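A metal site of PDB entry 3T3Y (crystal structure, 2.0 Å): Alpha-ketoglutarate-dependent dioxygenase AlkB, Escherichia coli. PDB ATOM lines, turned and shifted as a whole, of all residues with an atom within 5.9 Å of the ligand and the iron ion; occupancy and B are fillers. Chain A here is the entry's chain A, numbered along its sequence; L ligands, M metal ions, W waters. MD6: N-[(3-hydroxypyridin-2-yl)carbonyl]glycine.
Along chain A the residues within 4 Å of the iron ion span positions 121 to 177.
O of Leu 118 is in hydrogen-bond range of N of Ile 179 (3.0 Å). The guanidinium group (NH1) of Arg 173 is in hydrogen-bond range of the backbone carbonyl oxygen (O) of Asp 123 (2.6 Å). O of Arg 173 is in hydrogen-bond range of NE1 of Trp 168 (3.2 Å). The side-chain hydroxyl (OG) of Ser 135 sits at hydrogen-bond distance from the side-chain amide nitrogen (ND2) of Asn 196 (2.8 Å). The backbone carbonyl oxygen (O) of Asn 196 lies within hydrogen-bond range of the backbone NH (N) of Asn 110, at 2.9 Å. N of Tyr 112 lies within hydrogen-bond range of O of Arg 194, 2.9 Å away. The guanidinium group of Arg 200 lies within salt-bridge range of the side-chain carboxylate of Asp 123. The side-chain hydroxyl of Thr 198 lies within hydrogen-bond range of the guanidinium group of Arg 200 (2.8 Å).
The iron ion is bound by the side-chain carboxylate (OD1) of Asp 123 (2.1 Å), a nitrogen (N2) of the ligand (2.2 Å), an oxygen (O3) of the ligand (2.2 Å), water W1 (2.3 Å), a ring nitrogen (NE2) of His 177 (2.3 Å) and a ring nitrogen (NE2) of His 121 (2.3 Å). The iron ion has six donor atoms within binding distance.
O4 of the ligand is in hydrogen-bond range of OG of Ser 135, 2.7 Å away. An oxygen (O) of the ligand sits at hydrogen-bond distance from the side-chain amide nitrogen of Asn 196 (3.2 Å). The guanidinium group of Arg 194 is in salt-bridge range of an oxygen (OXT) of the ligand, at 2.7 Å. OXT of the ligand is in hydrogen-bond range of OH of Tyr 112 (2.6 Å).
Asn 110 touches the ligand. CD2 of Leu 118 touches O3 of the ligand (3.7 Å). Ile 133 touches the ligand (CG2 to C6, 3.7 Å). Phe 144 touches the ligand (CE1 to O4, 3.8 Å). Trp 168 touches the ligand (CG to C6, 3.4 Å). Ile 179 touches the ligand (CD1 to O, 3.5 Å). Thr 198 touches the ligand. Within 4 Å of the ligand: Asn 110, Tyr 112, Leu 118, His 121, Asp 123, Ile 133, Ser 135, Phe 144, Trp 168, His 177, Ile 179, Arg 194, Asn 196 and Thr 198. Along chain A the residues within 4 Å of the ligand span positions 110 to 198.
Water W1 bridges OD2 of Asp 123 and NH2 of Arg 200.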
ATOM      1  N   ASN A 110      -5.058  18.970  15.767  1.00  0.00           N
ATOM      2  CA  ASN A 110      -4.932  20.179  16.570  1.00  0.00           C
ATOM      3  C   ASN A 110      -5.917  21.235  16.069  1.00  0.00           C
ATOM      4  O   ASN A 110      -6.077  21.396  14.877  1.00  0.00           O
ATOM      5  CB  ASN A 110      -3.520  20.778  16.431  1.00  0.00           C
ATOM      6  CG  ASN A 110      -2.461  20.000  17.198  1.00  0.00           C
ATOM      7  OD1 ASN A 110      -2.777  19.039  17.878  1.00  0.00           O
ATOM      8  ND2 ASN A 110      -1.199  20.429  17.084  1.00  0.00           N
ATOM      9  N   TYR A 112      -6.667  25.416  16.543  1.00  0.00           N
ATOM     10  CA  TYR A 112      -6.151  26.664  17.082  1.00  0.00           C
ATOM     11  C   TYR A 112      -7.170  27.770  16.937  1.00  0.00           C
ATOM     12  O   TYR A 112      -7.549  28.109  15.819  1.00  0.00           O
ATOM     13  CB  TYR A 112      -4.894  27.122  16.302  1.00  0.00           C
ATOM     14  CG  TYR A 112      -3.720  26.189  16.413  1.00  0.00           C
ATOM     15  CD1 TYR A 112      -3.689  25.000  15.694  1.00  0.00           C
ATOM     16  CD2 TYR A 112      -2.639  26.500  17.224  1.00  0.00           C
ATOM     17  CE1 TYR A 112      -2.606  24.138  15.787  1.00  0.00           C
ATOM     18  CE2 TYR A 112      -1.553  25.657  17.325  1.00  0.00           C
ATOM     19  CZ  TYR A 112      -1.553  24.475  16.603  1.00  0.00           C
ATOM     20  OH  TYR A 112      -0.476  23.626  16.721  1.00  0.00           O
ATOM     21  N   LEU A 118       1.532  26.575  19.938  1.00  0.00           N
ATOM     22  CA  LEU A 118       2.047  25.289  20.369  1.00  0.00           C
ATOM     23  C   LEU A 118       3.512  25.460  20.769  1.00  0.00           C
ATOM     24  O   LEU A 118       4.354  25.870  19.961  1.00  0.00           O
ATOM     25  CB  LEU A 118       1.899  24.248  19.247  1.00  0.00           C
ATOM     26  CG  LEU A 118       2.320  22.815  19.575  1.00  0.00           C
ATOM     27  CD1 LEU A 118       1.347  22.186  20.584  1.00  0.00           C
ATOM     28  CD2 LEU A 118       2.387  21.974  18.307  1.00  0.00           C
ATOM     29  N   HIS A 121       8.822  21.870  20.989  1.00  0.00           N
ATOM     30  CA  HIS A 121       8.840  20.483  21.399  1.00  0.00           C
ATOM     31  C   HIS A 121       9.424  19.607  20.299  1.00  0.00           C
ATOM     32  O   HIS A 121       9.571  20.030  19.153  1.00  0.00           O
ATOM     33  CB  HIS A 121       7.409  20.024  21.682  1.00  0.00           C
ATOM     34  CG  HIS A 121       6.588  19.875  20.438  1.00  0.00           C
ATOM     35  ND1 HIS A 121       5.915  20.934  19.865  1.00  0.00           N
ATOM     36  CD2 HIS A 121       6.348  18.805  19.649  1.00  0.00           C
ATOM     37  CE1 HIS A 121       5.294  20.521  18.771  1.00  0.00           C
ATOM     38  NE2 HIS A 121       5.547  19.236  18.618  1.00  0.00           N
ATOM     39  N   GLN A 122       9.766  18.371  20.669  1.00  0.00           N
ATOM     40  CA  GLN A 122      10.158  17.349  19.710  1.00  0.00           C
ATOM     41  C   GLN A 122       9.090  16.278  19.703  1.00  0.00           C
ATOM     42  O   GLN A 122       8.463  16.006  20.728  1.00  0.00           O
ATOM     43  CB  GLN A 122      11.466  16.686  20.130  1.00  0.00           C
ATOM     44  CG  GLN A 122      12.629  17.587  20.426  1.00  0.00           C
ATOM     45  CD  GLN A 122      13.810  16.789  20.957  1.00  0.00           C
ATOM     46  OE1 GLN A 122      13.849  16.426  22.133  1.00  0.00           O
ATOM     47  NE2 GLN A 122      14.768  16.484  20.079  1.00  0.00           N
ATOM     48  N   ASP A 123       8.864  15.655  18.552  1.00  0.00           N
ATOM     49  CA  ASP A 123       8.096  14.417  18.508  1.00  0.00           C
ATOM     50  C   ASP A 123       9.061  13.235  18.524  1.00  0.00           C
ATOM     51  O   ASP A 123       9.569  12.816  17.481  1.00  0.00           O
ATOM     52  CB  ASP A 123       7.179  14.385  17.295  1.00  0.00           C
ATOM     53  CG  ASP A 123       6.080  15.421  17.369  1.00  0.00           C
ATOM     54  OD1 ASP A 123       6.345  16.567  16.972  1.00  0.00           O
ATOM     55  OD2 ASP A 123       4.973  15.104  17.837  1.00  0.00           O
ATOM     56  N   ILE A 133       6.829  12.275   9.824  1.00  0.00           N
ATOM     57  CA  ILE A 133       5.496  12.697  10.234  1.00  0.00           C
ATOM     58  C   ILE A 133       4.953  13.519   9.083  1.00  0.00           C
ATOM     59  O   ILE A 133       5.675  14.344   8.498  1.00  0.00           O
ATOM     60  CB  ILE A 133       5.534  13.482  11.557  1.00  0.00           C
ATOM     61  CG1 ILE A 133       5.839  12.531  12.708  1.00  0.00           C
ATOM     62  CG2 ILE A 133       4.201  14.211  11.828  1.00  0.00           C
ATOM     63  CD1 ILE A 133       5.932  13.217  14.054  1.00  0.00           C
ATOM     64  N   VAL A 134       3.692  13.265   8.727  1.00  0.00           N
ATOM     65  CA  VAL A 134       3.032  14.030   7.682  1.00  0.00           C
ATOM     66  C   VAL A 134       2.090  15.040   8.319  1.00  0.00           C
ATOM     67  O   VAL A 134       1.204  14.686   9.120  1.00  0.00           O
ATOM     68  CB  VAL A 134       2.256  13.122   6.697  1.00  0.00           C
ATOM     69  CG1 VAL A 134       1.517  13.948   5.650  1.00  0.00           C
ATOM     70  CG2 VAL A 134       3.204  12.124   6.031  1.00  0.00           C
ATOM     71  N   SER A 135       2.289  16.310   7.972  1.00  0.00           N
ATOM     72  CA  SER A 135       1.579  17.390   8.623  1.00  0.00           C
ATOM     73  C   SER A 135       0.790  18.237   7.626  1.00  0.00           C
ATOM     74  O   SER A 135       1.335  18.746   6.631  1.00  0.00           O
ATOM     75  CB  SER A 135       2.559  18.258   9.401  1.00  0.00           C
ATOM     76  OG  SER A 135       1.921  19.427   9.894  1.00  0.00           O
ATOM     77  N   SER A 137      -1.946  21.434   7.038  1.00  0.00           N
ATOM     78  CA  SER A 137      -2.499  22.688   7.548  1.00  0.00           C
ATOM     79  C   SER A 137      -3.787  23.044   6.834  1.00  0.00           C
ATOM     80  O   SER A 137      -3.877  22.929   5.604  1.00  0.00           O
ATOM     81  CB  SER A 137      -1.486  23.827   7.377  1.00  0.00           C
ATOM     82  OG  SER A 137      -0.387  23.673   8.251  1.00  0.00           O
ATOM     83  N   PHE A 144       5.178  28.633  11.555  1.00  0.00           N
ATOM     84  CA  PHE A 144       5.808  27.432  12.067  1.00  0.00           C
ATOM     85  C   PHE A 144       7.269  27.771  12.340  1.00  0.00           C
ATOM     86  O   PHE A 144       7.951  28.353  11.495  1.00  0.00           O
ATOM     87  CB  PHE A 144       5.670  26.316  11.011  1.00  0.00           C
ATOM     88  CG  PHE A 144       6.322  25.016  11.384  1.00  0.00           C
ATOM     89  CD1 PHE A 144       5.684  24.112  12.208  1.00  0.00           C
ATOM     90  CD2 PHE A 144       7.556  24.686  10.862  1.00  0.00           C
ATOM     91  CE1 PHE A 144       6.284  22.905  12.522  1.00  0.00           C
ATOM     92  CE2 PHE A 144       8.163  23.491  11.171  1.00  0.00           C
ATOM     93  CZ  PHE A 144       7.521  22.593  12.008  1.00  0.00           C
ATOM     94  N   LEU A 160       2.883  28.654   7.316  1.00  0.00           N
ATOM     95  CA  LEU A 160       2.115  27.553   6.740  1.00  0.00           C
ATOM     96  C   LEU A 160       0.693  28.023   6.455  1.00  0.00           C
ATOM     97  O   LEU A 160       0.020  28.613   7.314  1.00  0.00           O
ATOM     98  CB  LEU A 160       2.069  26.341   7.686  1.00  0.00           C
ATOM     99  CG  LEU A 160       3.380  25.641   8.012  1.00  0.00           C
ATOM    100  CD1 LEU A 160       3.146  24.512   9.009  1.00  0.00           C
ATOM    101  CD2 LEU A 160       4.042  25.107   6.732  1.00  0.00           C
ATOM    102  N   VAL A 166       3.512  19.408   5.021  1.00  0.00           N
ATOM    103  CA  VAL A 166       4.939  19.239   5.252  1.00  0.00           C
ATOM    104  C   VAL A 166       5.181  17.773   5.561  1.00  0.00           C
ATOM    105  O   VAL A 166       4.494  17.189   6.390  1.00  0.00           O
ATOM    106  CB  VAL A 166       5.400  20.086   6.443  1.00  0.00           C
ATOM    107  CG1 VAL A 166       6.874  19.812   6.763  1.00  0.00           C
ATOM    108  CG2 VAL A 166       5.167  21.597   6.154  1.00  0.00           C
ATOM    109  N   TRP A 168       7.812  15.672   7.287  1.00  0.00           N
ATOM    110  CA  TRP A 168       8.876  15.973   8.229  1.00  0.00           C
ATOM    111  C   TRP A 168       9.698  14.703   8.434  1.00  0.00           C
ATOM    112  O   TRP A 168       9.303  13.819   9.202  1.00  0.00           O
ATOM    113  CB  TRP A 168       8.214  16.402   9.547  1.00  0.00           C
ATOM    114  CG  TRP A 168       9.071  17.007  10.625  1.00  0.00           C
ATOM    115  CD1 TRP A 168       9.413  16.438  11.826  1.00  0.00           C
ATOM    116  CD2 TRP A 168       9.641  18.330  10.642  1.00  0.00           C
ATOM    117  NE1 TRP A 168      10.174  17.308  12.574  1.00  0.00           N
ATOM    118  CE2 TRP A 168      10.330  18.480  11.870  1.00  0.00           C
ATOM    119  CE3 TRP A 168       9.643  19.396   9.743  1.00  0.00           C
ATOM    120  CZ2 TRP A 168      11.025  19.641  12.219  1.00  0.00           C
ATOM    121  CZ3 TRP A 168      10.330  20.561  10.088  1.00  0.00           C
ATOM    122  CH2 TRP A 168      11.007  20.672  11.309  1.00  0.00           C
ATOM    123  N   ARG A 173      13.649  15.331  11.406  1.00  0.00           N
ATOM    124  CA  ARG A 173      12.688  14.518  12.146  1.00  0.00           C
ATOM    125  C   ARG A 173      12.670  14.836  13.644  1.00  0.00           C
ATOM    126  O   ARG A 173      11.599  15.004  14.232  1.00  0.00           O
ATOM    127  CB  ARG A 173      12.953  13.024  11.908  1.00  0.00           C
ATOM    128  CG  ARG A 173      12.000  12.087  12.623  1.00  0.00           C
ATOM    129  CD  ARG A 173      10.534  12.294  12.226  1.00  0.00           C
ATOM    130  NE  ARG A 173       9.703  11.391  13.011  1.00  0.00           N
ATOM    131  CZ  ARG A 173       9.331  11.632  14.267  1.00  0.00           C
ATOM    132  NH1 ARG A 173       9.696  12.773  14.839  1.00  0.00           N
ATOM    133  NH2 ARG A 173       8.598  10.759  14.939  1.00  0.00           N
ATOM    134  N   HIS A 177      10.385  22.175  17.407  1.00  0.00           N
ATOM    135  CA  HIS A 177       9.540  23.014  16.555  1.00  0.00           C
ATOM    136  C   HIS A 177       8.274  23.404  17.283  1.00  0.00           C
ATOM    137  O   HIS A 177       7.926  22.825  18.321  1.00  0.00           O
ATOM    138  CB  HIS A 177       9.165  22.271  15.267  1.00  0.00           C
ATOM    139  CG  HIS A 177       8.511  20.948  15.513  1.00  0.00           C
ATOM    140  ND1 HIS A 177       9.225  19.811  15.819  1.00  0.00           N
ATOM    141  CD2 HIS A 177       7.196  20.588  15.547  1.00  0.00           C
ATOM    142  CE1 HIS A 177       8.384  18.805  16.013  1.00  0.00           C
ATOM    143  NE2 HIS A 177       7.155  19.242  15.840  1.00  0.00           N
ATOM    144  N   ILE A 179       4.526  26.369  17.054  1.00  0.00           N
ATOM    145  CA  ILE A 179       3.655  27.273  16.317  1.00  0.00           C
ATOM    146  C   ILE A 179       3.471  28.556  17.121  1.00  0.00           C
ATOM    147  O   ILE A 179       3.161  28.510  18.320  1.00  0.00           O
ATOM    148  CB  ILE A 179       2.284  26.597  16.035  1.00  0.00           C
ATOM    149  CG1 ILE A 179       2.449  25.402  15.092  1.00  0.00           C
ATOM    150  CG2 ILE A 179       1.284  27.590  15.432  1.00  0.00           C
ATOM    151  CD1 ILE A 179       2.614  25.784  13.631  1.00  0.00           C
ATOM    152  N   ARG A 194      -7.525  27.386  12.824  1.00  0.00           N
ATOM    153  CA  ARG A 194      -6.630  26.619  11.987  1.00  0.00           C
ATOM    154  C   ARG A 194      -6.684  25.191  12.522  1.00  0.00           C
ATOM    155  O   ARG A 194      -6.726  24.977  13.725  1.00  0.00           O
ATOM    156  CB  ARG A 194      -5.207  27.140  12.092  1.00  0.00           C
ATOM    157  CG  ARG A 194      -4.174  26.205  11.472  1.00  0.00           C
ATOM    158  CD  ARG A 194      -2.784  26.788  11.603  1.00  0.00           C
ATOM    159  NE  ARG A 194      -1.790  25.936  10.963  1.00  0.00           N
ATOM    160  CZ  ARG A 194      -1.037  25.049  11.614  1.00  0.00           C
ATOM    161  NH1 ARG A 194      -1.124  24.938  12.932  1.00  0.00           N
ATOM    162  NH2 ARG A 194      -0.161  24.302  10.941  1.00  0.00           N
ATOM    163  N   ASN A 196      -4.635  21.439  12.243  1.00  0.00           N
ATOM    164  CA  ASN A 196      -3.457  20.741  11.772  1.00  0.00           C
ATOM    165  C   ASN A 196      -3.610  19.246  12.000  1.00  0.00           C
ATOM    166  O   ASN A 196      -4.032  18.819  13.081  1.00  0.00           O
ATOM    167  CB  ASN A 196      -2.191  21.283  12.454  1.00  0.00           C
ATOM    168  CG  ASN A 196      -0.968  20.454  12.134  1.00  0.00           C
ATOM    169  OD1 ASN A 196      -0.507  19.680  12.965  1.00  0.00           O
ATOM    170  ND2 ASN A 196      -0.411  20.626  10.940  1.00  0.00           N
ATOM    171  N   THR A 198      -1.408  15.742  12.071  1.00  0.00           N
ATOM    172  CA  THR A 198      -0.097  15.103  12.009  1.00  0.00           C
ATOM    173  C   THR A 198      -0.254  13.592  12.049  1.00  0.00           C
ATOM    174  O   THR A 198      -0.706  13.021  13.041  1.00  0.00           O
ATOM    175  CB  THR A 198       0.917  15.567  13.107  1.00  0.00           C
ATOM    176  OG1 THR A 198       0.266  15.633  14.385  1.00  0.00           O
ATOM    177  CG2 THR A 198       1.518  16.920  12.768  1.00  0.00           C
ATOM    178  N   ARG A 200       1.219   9.775  11.980  1.00  0.00           N
ATOM    179  CA  ARG A 200       2.354   9.104  12.597  1.00  0.00           C
ATOM    180  C   ARG A 200       2.260   7.589  12.517  1.00  0.00           C
ATOM    181  O   ARG A 200       1.169   7.021  12.540  1.00  0.00           O
ATOM    182  CB  ARG A 200       2.449   9.491  14.087  1.00  0.00           C
ATOM    183  CG  ARG A 200       2.438  11.003  14.347  1.00  0.00           C
ATOM    184  CD  ARG A 200       1.376  11.387  15.370  1.00  0.00           C
ATOM    185  NE  ARG A 200       1.297  12.839  15.570  1.00  0.00           N
ATOM    186  CZ  ARG A 200       2.227  13.537  16.204  1.00  0.00           C
ATOM    187  NH1 ARG A 200       3.304  12.941  16.705  1.00  0.00           N
ATOM    188  NH2 ARG A 200       2.089  14.852  16.338  1.00  0.00           N
HETATM  189  C   MD6 L   1       1.059  22.402  13.812  1.00  0.00           C
HETATM  190  N   MD6 L   1       2.736  20.697  13.854  1.00  0.00           N
HETATM  191  O   MD6 L   1       1.401  22.652  12.567  1.00  0.00           O
HETATM  192  CA  MD6 L   1       1.934  21.507  14.651  1.00  0.00           C
HETATM  193  N2  MD6 L   1       5.250  18.033  14.319  1.00  0.00           N
HETATM  194  OXT MD6 L   1       0.015  22.852  14.279  1.00  0.00           O
HETATM  195  C3  MD6 L   1       3.687  19.830  14.470  1.00  0.00           C
HETATM  196  O3  MD6 L   1       3.747  19.807  15.697  1.00  0.00           O
HETATM  197  C4  MD6 L   1       4.536  18.957  13.667  1.00  0.00           C
HETATM  198  O4  MD6 L   1       3.857  20.086  11.686  1.00  0.00           O
HETATM  199  C5  MD6 L   1       6.030  17.186  13.641  1.00  0.00           C
HETATM  200  C6  MD6 L   1       6.135  17.284  12.270  1.00  0.00           C
HETATM  201  C7  MD6 L   1       5.408  18.265  11.569  1.00  0.00           C
HETATM  202  C8  MD6 L   1       4.584  19.113  12.293  1.00  0.00           C
HETATM  203 FE    FE M   1       5.212  18.323  16.541  1.00  0.00          FE
HETATM  204  O   HOH W   1       3.370  17.179  17.179  1.00  0.00           O
HETATM  205  O   HOH W   2       5.076  21.237   9.789  1.00  0.00           O
